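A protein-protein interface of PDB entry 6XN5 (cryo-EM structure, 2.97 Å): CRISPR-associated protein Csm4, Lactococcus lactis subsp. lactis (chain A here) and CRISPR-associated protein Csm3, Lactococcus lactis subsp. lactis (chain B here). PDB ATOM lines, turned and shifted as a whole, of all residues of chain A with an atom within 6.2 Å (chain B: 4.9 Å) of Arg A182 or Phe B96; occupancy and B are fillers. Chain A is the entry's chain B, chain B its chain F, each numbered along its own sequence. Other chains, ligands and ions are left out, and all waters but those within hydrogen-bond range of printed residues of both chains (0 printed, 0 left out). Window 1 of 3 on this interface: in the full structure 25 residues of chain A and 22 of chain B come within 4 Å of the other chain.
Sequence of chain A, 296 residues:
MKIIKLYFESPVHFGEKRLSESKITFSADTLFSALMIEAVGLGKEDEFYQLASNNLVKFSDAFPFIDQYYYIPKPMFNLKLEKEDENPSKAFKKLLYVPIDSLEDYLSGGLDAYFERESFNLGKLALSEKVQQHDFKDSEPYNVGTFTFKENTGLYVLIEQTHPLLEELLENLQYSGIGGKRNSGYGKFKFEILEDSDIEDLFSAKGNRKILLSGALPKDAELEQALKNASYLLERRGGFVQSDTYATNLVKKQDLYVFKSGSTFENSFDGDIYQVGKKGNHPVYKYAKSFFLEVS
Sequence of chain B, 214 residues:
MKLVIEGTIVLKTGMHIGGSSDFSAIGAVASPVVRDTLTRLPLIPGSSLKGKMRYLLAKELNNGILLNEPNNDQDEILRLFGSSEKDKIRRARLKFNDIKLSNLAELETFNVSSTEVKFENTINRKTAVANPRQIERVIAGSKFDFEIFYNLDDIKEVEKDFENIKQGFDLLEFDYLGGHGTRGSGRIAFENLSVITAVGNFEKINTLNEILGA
OG of Ser A184 lies within hydrogen-bond range of NZ of Lys B50 (3.3 Å).
The backbone carbonyl oxygen (O) of Phe B96 lies within hydrogen-bond range of the backbone NH (N) of Gly A185 (3.1 Å).
N of Phe B96 lies within hydrogen-bond range of O of Asn A183, at 3.4 Å.
N of Asp B98 sits at hydrogen-bond distance from O of Gly A185 (3.0 Å).
The side-chain amino group of Lys B95 is in hydrogen-bond range of the backbone carbonyl oxygen of Tyr A186 (3.1 Å).
The backbone carbonyl oxygen of Ser A176 lies within hydrogen-bond range of the guanidinium group of Arg A182, 2.6 Å away.
N of Gly B46 lies within hydrogen-bond range of OD1 of Asp B98, at 2.8 Å.
The side-chain hydroxyl of Ser A176 sits at hydrogen-bond distance from the side-chain carboxylate of Glu A38.
The backbone NH (N) of Tyr A186 lies close to the backbone carbonyl oxygen (O) of Lys A181 (3.5 Å).
The side-chain amide oxygen of Asn B97 sits at hydrogen-bond distance from the side-chain amino group of Lys B95 (2.5 Å).
Among the printed residues, merely in contact across the chains: Ser A176 with Lys B95, Gly A177 with Lys B95, Arg A182 with Lys B95, Arg A182 with Phe B96, Asn A183 with Lys B50, Asn A183 with Leu B94, Asn A183 with Lys B95, Gly A185 with Asn B97 and Tyr A186 with Asp B98.
Of the printed residues of chain B, Ser A176 touches Lys B95.
Arg A182 touches just these residues of chain B: Lys B95 (3.2 Å) and Phe B96 (3.6 Å).
Of the printed residues of chain B, Ser A184 touches Lys B50.
Of chain A, only Arg A182 (3.6 Å), Asn A183 (3.4 Å) and Gly A185 (3.1 Å) come within 4 Å of Phe B96.
Ile B148 touches none of the printed residues of chain A.
The nearest residue of chain B that does not touch Arg A182 is Arg B91 (4.5 Å).
Hydrophobic or aromatic side chains of chain B that line the printed part of chain A: Phe B96.
Of the 15 printed residues of chain A, 7 touch a printed residue of chain B.
Hydrophobic or aromatic side chains of chain A within 4 Å of the printed part of chain B: Tyr A186.
Among the printed residues, 14 pairs touch across the chains.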
ATOM      1  N   ILE A  37     -17.070  -0.316 -12.532  1.00  0.00           N
ATOM      2  CA  ILE A  37     -16.534   1.017 -12.798  1.00  0.00           C
ATOM      3  C   ILE A  37     -16.600   1.332 -14.291  1.00  0.00           C
ATOM      4  O   ILE A  37     -16.931   2.454 -14.697  1.00  0.00           O
ATOM      5  CB  ILE A  37     -15.108   1.124 -12.231  1.00  0.00           C
ATOM      6  CG1 ILE A  37     -15.182   1.243 -10.717  1.00  0.00           C
ATOM      7  CG2 ILE A  37     -14.369   2.320 -12.768  1.00  0.00           C
ATOM      8  CD1 ILE A  37     -13.912   0.923 -10.026  1.00  0.00           C
ATOM      9  N   GLU A  38     -16.346   0.337 -15.134  1.00  0.00           N
ATOM     10  CA  GLU A  38     -16.542   0.578 -16.556  1.00  0.00           C
ATOM     11  C   GLU A  38     -18.007   0.674 -16.945  1.00  0.00           C
ATOM     12  O   GLU A  38     -18.313   1.254 -17.988  1.00  0.00           O
ATOM     13  CB  GLU A  38     -15.848  -0.504 -17.370  1.00  0.00           C
ATOM     14  CG  GLU A  38     -14.356  -0.432 -17.208  1.00  0.00           C
ATOM     15  CD  GLU A  38     -13.770   0.836 -17.804  1.00  0.00           C
ATOM     16  OE1 GLU A  38     -14.312   1.348 -18.807  1.00  0.00           O
ATOM     17  OE2 GLU A  38     -12.794   1.356 -17.231  1.00  0.00           O
ATOM     18  N   SER A 176      -8.313   0.365 -20.161  1.00  0.00           N
ATOM     19  CA  SER A 176      -8.352   1.116 -18.915  1.00  0.00           C
ATOM     20  C   SER A 176      -7.415   0.580 -17.856  1.00  0.00           C
ATOM     21  O   SER A 176      -6.894   1.356 -17.061  1.00  0.00           O
ATOM     22  CB  SER A 176      -9.766   1.120 -18.350  1.00  0.00           C
ATOM     23  OG  SER A 176      -9.861   1.984 -17.240  1.00  0.00           O
ATOM     24  N   GLY A 177      -7.214  -0.728 -17.806  1.00  0.00           N
ATOM     25  CA  GLY A 177      -6.296  -1.314 -16.855  1.00  0.00           C
ATOM     26  C   GLY A 177      -6.966  -2.160 -15.796  1.00  0.00           C
ATOM     27  O   GLY A 177      -8.054  -1.831 -15.319  1.00  0.00           O
ATOM     28  N   ILE A 178      -6.322  -3.255 -15.419  1.00  0.00           N
ATOM     29  CA  ILE A 178      -6.792  -4.124 -14.352  1.00  0.00           C
ATOM     30  C   ILE A 178      -5.742  -4.124 -13.249  1.00  0.00           C
ATOM     31  O   ILE A 178      -4.539  -4.068 -13.520  1.00  0.00           O
ATOM     32  CB  ILE A 178      -7.115  -5.549 -14.875  1.00  0.00           C
ATOM     33  CG1 ILE A 178      -7.837  -6.393 -13.824  1.00  0.00           C
ATOM     34  CG2 ILE A 178      -5.897  -6.263 -15.428  1.00  0.00           C
ATOM     35  CD1 ILE A 178      -9.198  -5.914 -13.479  1.00  0.00           C
ATOM     36  N   GLY A 179      -6.196  -4.094 -12.009  1.00  0.00           N
ATOM     37  CA  GLY A 179      -5.297  -4.076 -10.883  1.00  0.00           C
ATOM     38  C   GLY A 179      -5.048  -2.686 -10.345  1.00  0.00           C
ATOM     39  O   GLY A 179      -5.827  -1.755 -10.539  1.00  0.00           O
ATOM     40  N   GLY A 180      -3.936  -2.558  -9.644  1.00  0.00           N
ATOM     41  CA  GLY A 180      -3.574  -1.318  -9.004  1.00  0.00           C
ATOM     42  C   GLY A 180      -2.450  -0.621  -9.733  1.00  0.00           C
ATOM     43  O   GLY A 180      -1.690  -1.257 -10.456  1.00  0.00           O
ATOM     44  N   LYS A 181      -2.361   0.694  -9.507  1.00  0.00           N
ATOM     45  CA  LYS A 181      -1.454   1.605 -10.217  1.00  0.00           C
ATOM     46  C   LYS A 181      -1.616   1.489 -11.724  1.00  0.00           C
ATOM     47  O   LYS A 181      -0.640   1.439 -12.468  1.00  0.00           O
ATOM     48  CB  LYS A 181       0.006   1.386  -9.821  1.00  0.00           C
ATOM     49  CG  LYS A 181       0.358   1.830  -8.437  1.00  0.00           C
ATOM     50  CD  LYS A 181       0.308   3.322  -8.325  1.00  0.00           C
ATOM     51  CE  LYS A 181       0.808   3.756  -6.984  1.00  0.00           C
ATOM     52  NZ  LYS A 181       0.388   5.125  -6.650  1.00  0.00           N
ATOM     53  N   ARG A 182      -2.863   1.428 -12.181  1.00  0.00           N
ATOM     54  CA  ARG A 182      -3.108   1.195 -13.598  1.00  0.00           C
ATOM     55  C   ARG A 182      -2.837   2.447 -14.427  1.00  0.00           C
ATOM     56  O   ARG A 182      -2.301   2.357 -15.534  1.00  0.00           O
ATOM     57  CB  ARG A 182      -4.531   0.682 -13.798  1.00  0.00           C
ATOM     58  CG  ARG A 182      -5.553   1.488 -13.064  1.00  0.00           C
ATOM     59  CD  ARG A 182      -6.879   0.801 -12.990  1.00  0.00           C
ATOM     60  NE  ARG A 182      -7.967   1.750 -12.780  1.00  0.00           N
ATOM     61  CZ  ARG A 182      -8.497   2.517 -13.726  1.00  0.00           C
ATOM     62  NH1 ARG A 182      -8.060   2.452 -14.974  1.00  0.00           N
ATOM     63  NH2 ARG A 182      -9.484   3.345 -13.425  1.00  0.00           N
ATOM     64  N   ASN A 183      -3.148   3.623 -13.895  1.00  0.00           N
ATOM     65  CA  ASN A 183      -2.858   4.869 -14.588  1.00  0.00           C
ATOM     66  C   ASN A 183      -1.395   5.253 -14.517  1.00  0.00           C
ATOM     67  O   ASN A 183      -0.982   6.190 -15.203  1.00  0.00           O
ATOM     68  CB  ASN A 183      -3.694   5.999 -14.005  1.00  0.00           C
ATOM     69  CG  ASN A 183      -5.150   5.676 -13.982  1.00  0.00           C
ATOM     70  OD1 ASN A 183      -5.716   5.244 -14.979  1.00  0.00           O
ATOM     71  ND2 ASN A 183      -5.772   5.862 -12.832  1.00  0.00           N
ATOM     72  N   SER A 184      -0.604   4.557 -13.704  1.00  0.00           N
ATOM     73  CA  SER A 184       0.807   4.867 -13.526  1.00  0.00           C
ATOM     74  C   SER A 184       1.704   3.817 -14.166  1.00  0.00           C
ATOM     75  O   SER A 184       2.817   3.595 -13.691  1.00  0.00           O
ATOM     76  CB  SER A 184       1.137   5.004 -12.041  1.00  0.00           C
ATOM     77  OG  SER A 184       0.314   5.986 -11.437  1.00  0.00           O
ATOM     78  N   GLY A 185       1.238   3.153 -15.218  1.00  0.00           N
ATOM     79  CA  GLY A 185       2.131   2.340 -16.013  1.00  0.00           C
ATOM     80  C   GLY A 185       1.845   0.859 -16.090  1.00  0.00           C
ATOM     81  O   GLY A 185       2.577   0.135 -16.765  1.00  0.00           O
ATOM     82  N   TYR A 186       0.807   0.380 -15.419  1.00  0.00           N
ATOM     83  CA  TYR A 186       0.629  -1.051 -15.223  1.00  0.00           C
ATOM     84  C   TYR A 186      -0.714  -1.524 -15.754  1.00  0.00           C
ATOM     85  O   TYR A 186      -1.614  -0.735 -16.041  1.00  0.00           O
ATOM     86  CB  TYR A 186       0.751  -1.407 -13.739  1.00  0.00           C
ATOM     87  CG  TYR A 186       2.107  -1.101 -13.182  1.00  0.00           C
ATOM     88  CD1 TYR A 186       3.244  -1.326 -13.932  1.00  0.00           C
ATOM     89  CD2 TYR A 186       2.252  -0.545 -11.931  1.00  0.00           C
ATOM     90  CE1 TYR A 186       4.483  -1.035 -13.444  1.00  0.00           C
ATOM     91  CE2 TYR A 186       3.493  -0.247 -11.437  1.00  0.00           C
ATOM     92  CZ  TYR A 186       4.600  -0.496 -12.201  1.00  0.00           C
ATOM     93  OH  TYR A 186       5.842  -0.206 -11.725  1.00  0.00           O
ATOM     94  N   GLY A 187      -0.821  -2.836 -15.907  1.00  0.00           N
ATOM     95  CA  GLY A 187      -2.116  -3.468 -15.975  1.00  0.00           C
ATOM     96  C   GLY A 187      -2.774  -3.662 -17.320  1.00  0.00           C
ATOM     97  O   GLY A 187      -3.849  -4.260 -17.368  1.00  0.00           O
ATOM     98  N   GLN A 242     -12.941   3.007  -4.478  1.00  0.00           N
ATOM     99  CA  GLN A 242     -12.374   3.689  -5.636  1.00  0.00           C
ATOM    100  C   GLN A 242     -13.529   4.273  -6.440  1.00  0.00           C
ATOM    101  O   GLN A 242     -14.209   3.555  -7.177  1.00  0.00           O
ATOM    102  CB  GLN A 242     -11.535   2.720  -6.463  1.00  0.00           C
ATOM    103  CG  GLN A 242     -11.092   3.238  -7.815  1.00  0.00           C
ATOM    104  CD  GLN A 242     -10.027   2.383  -8.427  1.00  0.00           C
ATOM    105  OE1 GLN A 242      -9.329   1.657  -7.735  1.00  0.00           O
ATOM    106  NE2 GLN A 242      -9.901   2.450  -9.741  1.00  0.00           N
ATOM    107  N   GLY B  46       6.130   4.213 -17.126  1.00  0.00           N
ATOM    108  CA  GLY B  46       5.034   5.124 -17.379  1.00  0.00           C
ATOM    109  C   GLY B  46       4.897   6.163 -16.296  1.00  0.00           C
ATOM    110  O   GLY B  46       4.403   7.267 -16.548  1.00  0.00           O
ATOM    111  N   LEU B  49       7.492   9.146 -17.224  1.00  0.00           N
ATOM    112  CA  LEU B  49       6.950   9.997 -18.275  1.00  0.00           C
ATOM    113  C   LEU B  49       5.771  10.803 -17.765  1.00  0.00           C
ATOM    114  O   LEU B  49       5.690  12.016 -17.995  1.00  0.00           O
ATOM    115  CB  LEU B  49       6.528   9.142 -19.461  1.00  0.00           C
ATOM    116  CG  LEU B  49       6.037   9.931 -20.661  1.00  0.00           C
ATOM    117  CD1 LEU B  49       7.215  10.582 -21.320  1.00  0.00           C
ATOM    118  CD2 LEU B  49       5.316   9.030 -21.633  1.00  0.00           C
ATOM    119  N   LYS B  50       4.877  10.145 -17.021  1.00  0.00           N
ATOM    120  CA  LYS B  50       3.698  10.802 -16.476  1.00  0.00           C
ATOM    121  C   LYS B  50       4.072  11.905 -15.499  1.00  0.00           C
ATOM    122  O   LYS B  50       3.544  13.018 -15.577  1.00  0.00           O
ATOM    123  CB  LYS B  50       2.813   9.766 -15.797  1.00  0.00           C
ATOM    124  CG  LYS B  50       1.637  10.343 -15.068  1.00  0.00           C
ATOM    125  CD  LYS B  50       0.760   9.249 -14.549  1.00  0.00           C
ATOM    126  CE  LYS B  50       0.496   9.461 -13.105  1.00  0.00           C
ATOM    127  NZ  LYS B  50      -0.802   8.888 -12.679  1.00  0.00           N
ATOM    128  N   MET B  53       5.878  14.939 -17.306  1.00  0.00           N
ATOM    129  CA  MET B  53       4.864  15.740 -17.987  1.00  0.00           C
ATOM    130  C   MET B  53       4.012  16.531 -17.008  1.00  0.00           C
ATOM    131  O   MET B  53       3.702  17.698 -17.265  1.00  0.00           O
ATOM    132  CB  MET B  53       3.957  14.873 -18.850  1.00  0.00           C
ATOM    133  CG  MET B  53       4.588  14.234 -20.039  1.00  0.00           C
ATOM    134  SD  MET B  53       3.331  13.219 -20.813  1.00  0.00           S
ATOM    135  CE  MET B  53       2.260  14.495 -21.459  1.00  0.00           C
ATOM    136  N   PHE B  81      -4.527  14.499 -14.762  1.00  0.00           N
ATOM    137  CA  PHE B  81      -3.615  13.581 -14.104  1.00  0.00           C
ATOM    138  C   PHE B  81      -4.144  12.993 -12.810  1.00  0.00           C
ATOM    139  O   PHE B  81      -3.431  12.210 -12.180  1.00  0.00           O
ATOM    140  CB  PHE B  81      -2.283  14.277 -13.810  1.00  0.00           C
ATOM    141  CG  PHE B  81      -1.472  14.557 -15.027  1.00  0.00           C
ATOM    142  CD1 PHE B  81      -0.607  13.610 -15.525  1.00  0.00           C
ATOM    143  CD2 PHE B  81      -1.583  15.768 -15.679  1.00  0.00           C
ATOM    144  CE1 PHE B  81       0.133  13.866 -16.643  1.00  0.00           C
ATOM    145  CE2 PHE B  81      -0.845  16.025 -16.801  1.00  0.00           C
ATOM    146  CZ  PHE B  81       0.017  15.073 -17.283  1.00  0.00           C
ATOM    147  N   ARG B  91     -10.812  11.205 -10.932  1.00  0.00           N
ATOM    148  CA  ARG B  91     -10.177  10.162 -11.718  1.00  0.00           C
ATOM    149  C   ARG B  91      -9.309  10.792 -12.791  1.00  0.00           C
ATOM    150  O   ARG B  91      -9.702  11.770 -13.431  1.00  0.00           O
ATOM    151  CB  ARG B  91     -11.215   9.242 -12.350  1.00  0.00           C
ATOM    152  CG  ARG B  91     -12.025   8.470 -11.340  1.00  0.00           C
ATOM    153  CD  ARG B  91     -13.161   7.704 -11.987  1.00  0.00           C
ATOM    154  NE  ARG B  91     -12.698   6.831 -13.057  1.00  0.00           N
ATOM    155  CZ  ARG B  91     -13.411   6.545 -14.140  1.00  0.00           C
ATOM    156  NH1 ARG B  91     -14.614   7.074 -14.297  1.00  0.00           N
ATOM    157  NH2 ARG B  91     -12.919   5.737 -15.066  1.00  0.00           N
ATOM    158  N   LEU B  94      -5.795  10.317 -18.252  1.00  0.00           N
ATOM    159  CA  LEU B  94      -4.748   9.667 -19.012  1.00  0.00           C
ATOM    160  C   LEU B  94      -4.331   8.371 -18.338  1.00  0.00           C
ATOM    161  O   LEU B  94      -4.171   8.318 -17.117  1.00  0.00           O
ATOM    162  CB  LEU B  94      -3.541  10.587 -19.142  1.00  0.00           C
ATOM    163  CG  LEU B  94      -3.623  11.758 -20.102  1.00  0.00           C
ATOM    164  CD1 LEU B  94      -2.469  12.681 -19.828  1.00  0.00           C
ATOM    165  CD2 LEU B  94      -3.567  11.245 -21.508  1.00  0.00           C
ATOM    166  N   LYS B  95      -4.138   7.333 -19.142  1.00  0.00           N
ATOM    167  CA  LYS B  95      -3.698   6.027 -18.664  1.00  0.00           C
ATOM    168  C   LYS B  95      -2.343   5.764 -19.301  1.00  0.00           C
ATOM    169  O   LYS B  95      -2.263   5.295 -20.435  1.00  0.00           O
ATOM    170  CB  LYS B  95      -4.709   4.952 -19.019  1.00  0.00           C
ATOM    171  CG  LYS B  95      -4.604   3.658 -18.239  1.00  0.00           C
ATOM    172  CD  LYS B  95      -3.745   2.635 -18.934  1.00  0.00           C
ATOM    173  CE  LYS B  95      -3.757   1.319 -18.207  1.00  0.00           C
ATOM    174  NZ  LYS B  95      -2.724   0.409 -18.724  1.00  0.00           N
ATOM    175  N   PHE B  96      -1.278   6.059 -18.571  1.00  0.00           N
ATOM    176  CA  PHE B  96       0.073   5.846 -19.061  1.00  0.00           C
ATOM    177  C   PHE B  96       0.448   4.383 -18.884  1.00  0.00           C
ATOM    178  O   PHE B  96      -0.036   3.718 -17.969  1.00  0.00           O
ATOM    179  CB  PHE B  96       1.060   6.735 -18.311  1.00  0.00           C
ATOM    180  CG  PHE B  96       0.959   8.195 -18.654  1.00  0.00           C
ATOM    181  CD1 PHE B  96      -0.009   8.992 -18.079  1.00  0.00           C
ATOM    182  CD2 PHE B  96       1.858   8.779 -19.517  1.00  0.00           C
ATOM    183  CE1 PHE B  96      -0.090  10.326 -18.377  1.00  0.00           C
ATOM    184  CE2 PHE B  96       1.776  10.117 -19.809  1.00  0.00           C
ATOM    185  CZ  PHE B  96       0.798  10.884 -19.243  1.00  0.00           C
ATOM    186  N   ASN B  97       1.308   3.885 -19.766  1.00  0.00           N
ATOM    187  CA  ASN B  97       1.793   2.513 -19.707  1.00  0.00           C
ATOM    188  C   ASN B  97       3.311   2.507 -19.730  1.00  0.00           C
ATOM    189  O   ASN B  97       3.929   3.430 -20.258  1.00  0.00           O
ATOM    190  CB  ASN B  97       1.260   1.685 -20.865  1.00  0.00           C
ATOM    191  CG  ASN B  97      -0.225   1.811 -21.019  1.00  0.00           C
ATOM    192  OD1 ASN B  97      -0.976   1.323 -20.186  1.00  0.00           O
ATOM    193  ND2 ASN B  97      -0.663   2.478 -22.071  1.00  0.00           N
ATOM    194  N   ASP B  98       3.904   1.472 -19.137  1.00  0.00           N
ATOM    195  CA  ASP B  98       5.351   1.320 -19.170  1.00  0.00           C
ATOM    196  C   ASP B  98       5.812   1.042 -20.589  1.00  0.00           C
ATOM    197  O   ASP B  98       5.248   0.197 -21.288  1.00  0.00           O
ATOM    198  CB  ASP B  98       5.800   0.193 -18.245  1.00  0.00           C
ATOM    199  CG  ASP B  98       6.028   0.662 -16.828  1.00  0.00           C
ATOM    200  OD1 ASP B  98       5.371   1.635 -16.412  1.00  0.00           O
ATOM    201  OD2 ASP B  98       6.868   0.061 -16.128  1.00  0.00           O
ATOM    202  N   ILE B 148      -0.721   5.756 -24.826  1.00  0.00           N
ATOM    203  CA  ILE B 148      -1.308   6.320 -23.622  1.00  0.00           C
ATOM    204  C   ILE B 148      -2.803   6.392 -23.867  1.00  0.00           C
ATOM    205  O   ILE B 148      -3.237   6.856 -24.924  1.00  0.00           O
ATOM    206  CB  ILE B 148      -0.730   7.716 -23.330  1.00  0.00           C
ATOM    207  CG1 ILE B 148       0.775   7.647 -23.127  1.00  0.00           C
ATOM    208  CG2 ILE B 148      -1.347   8.300 -22.092  1.00  0.00           C
ATOM    209  CD1 ILE B 148       1.415   8.992 -23.149  1.00  0.00           C
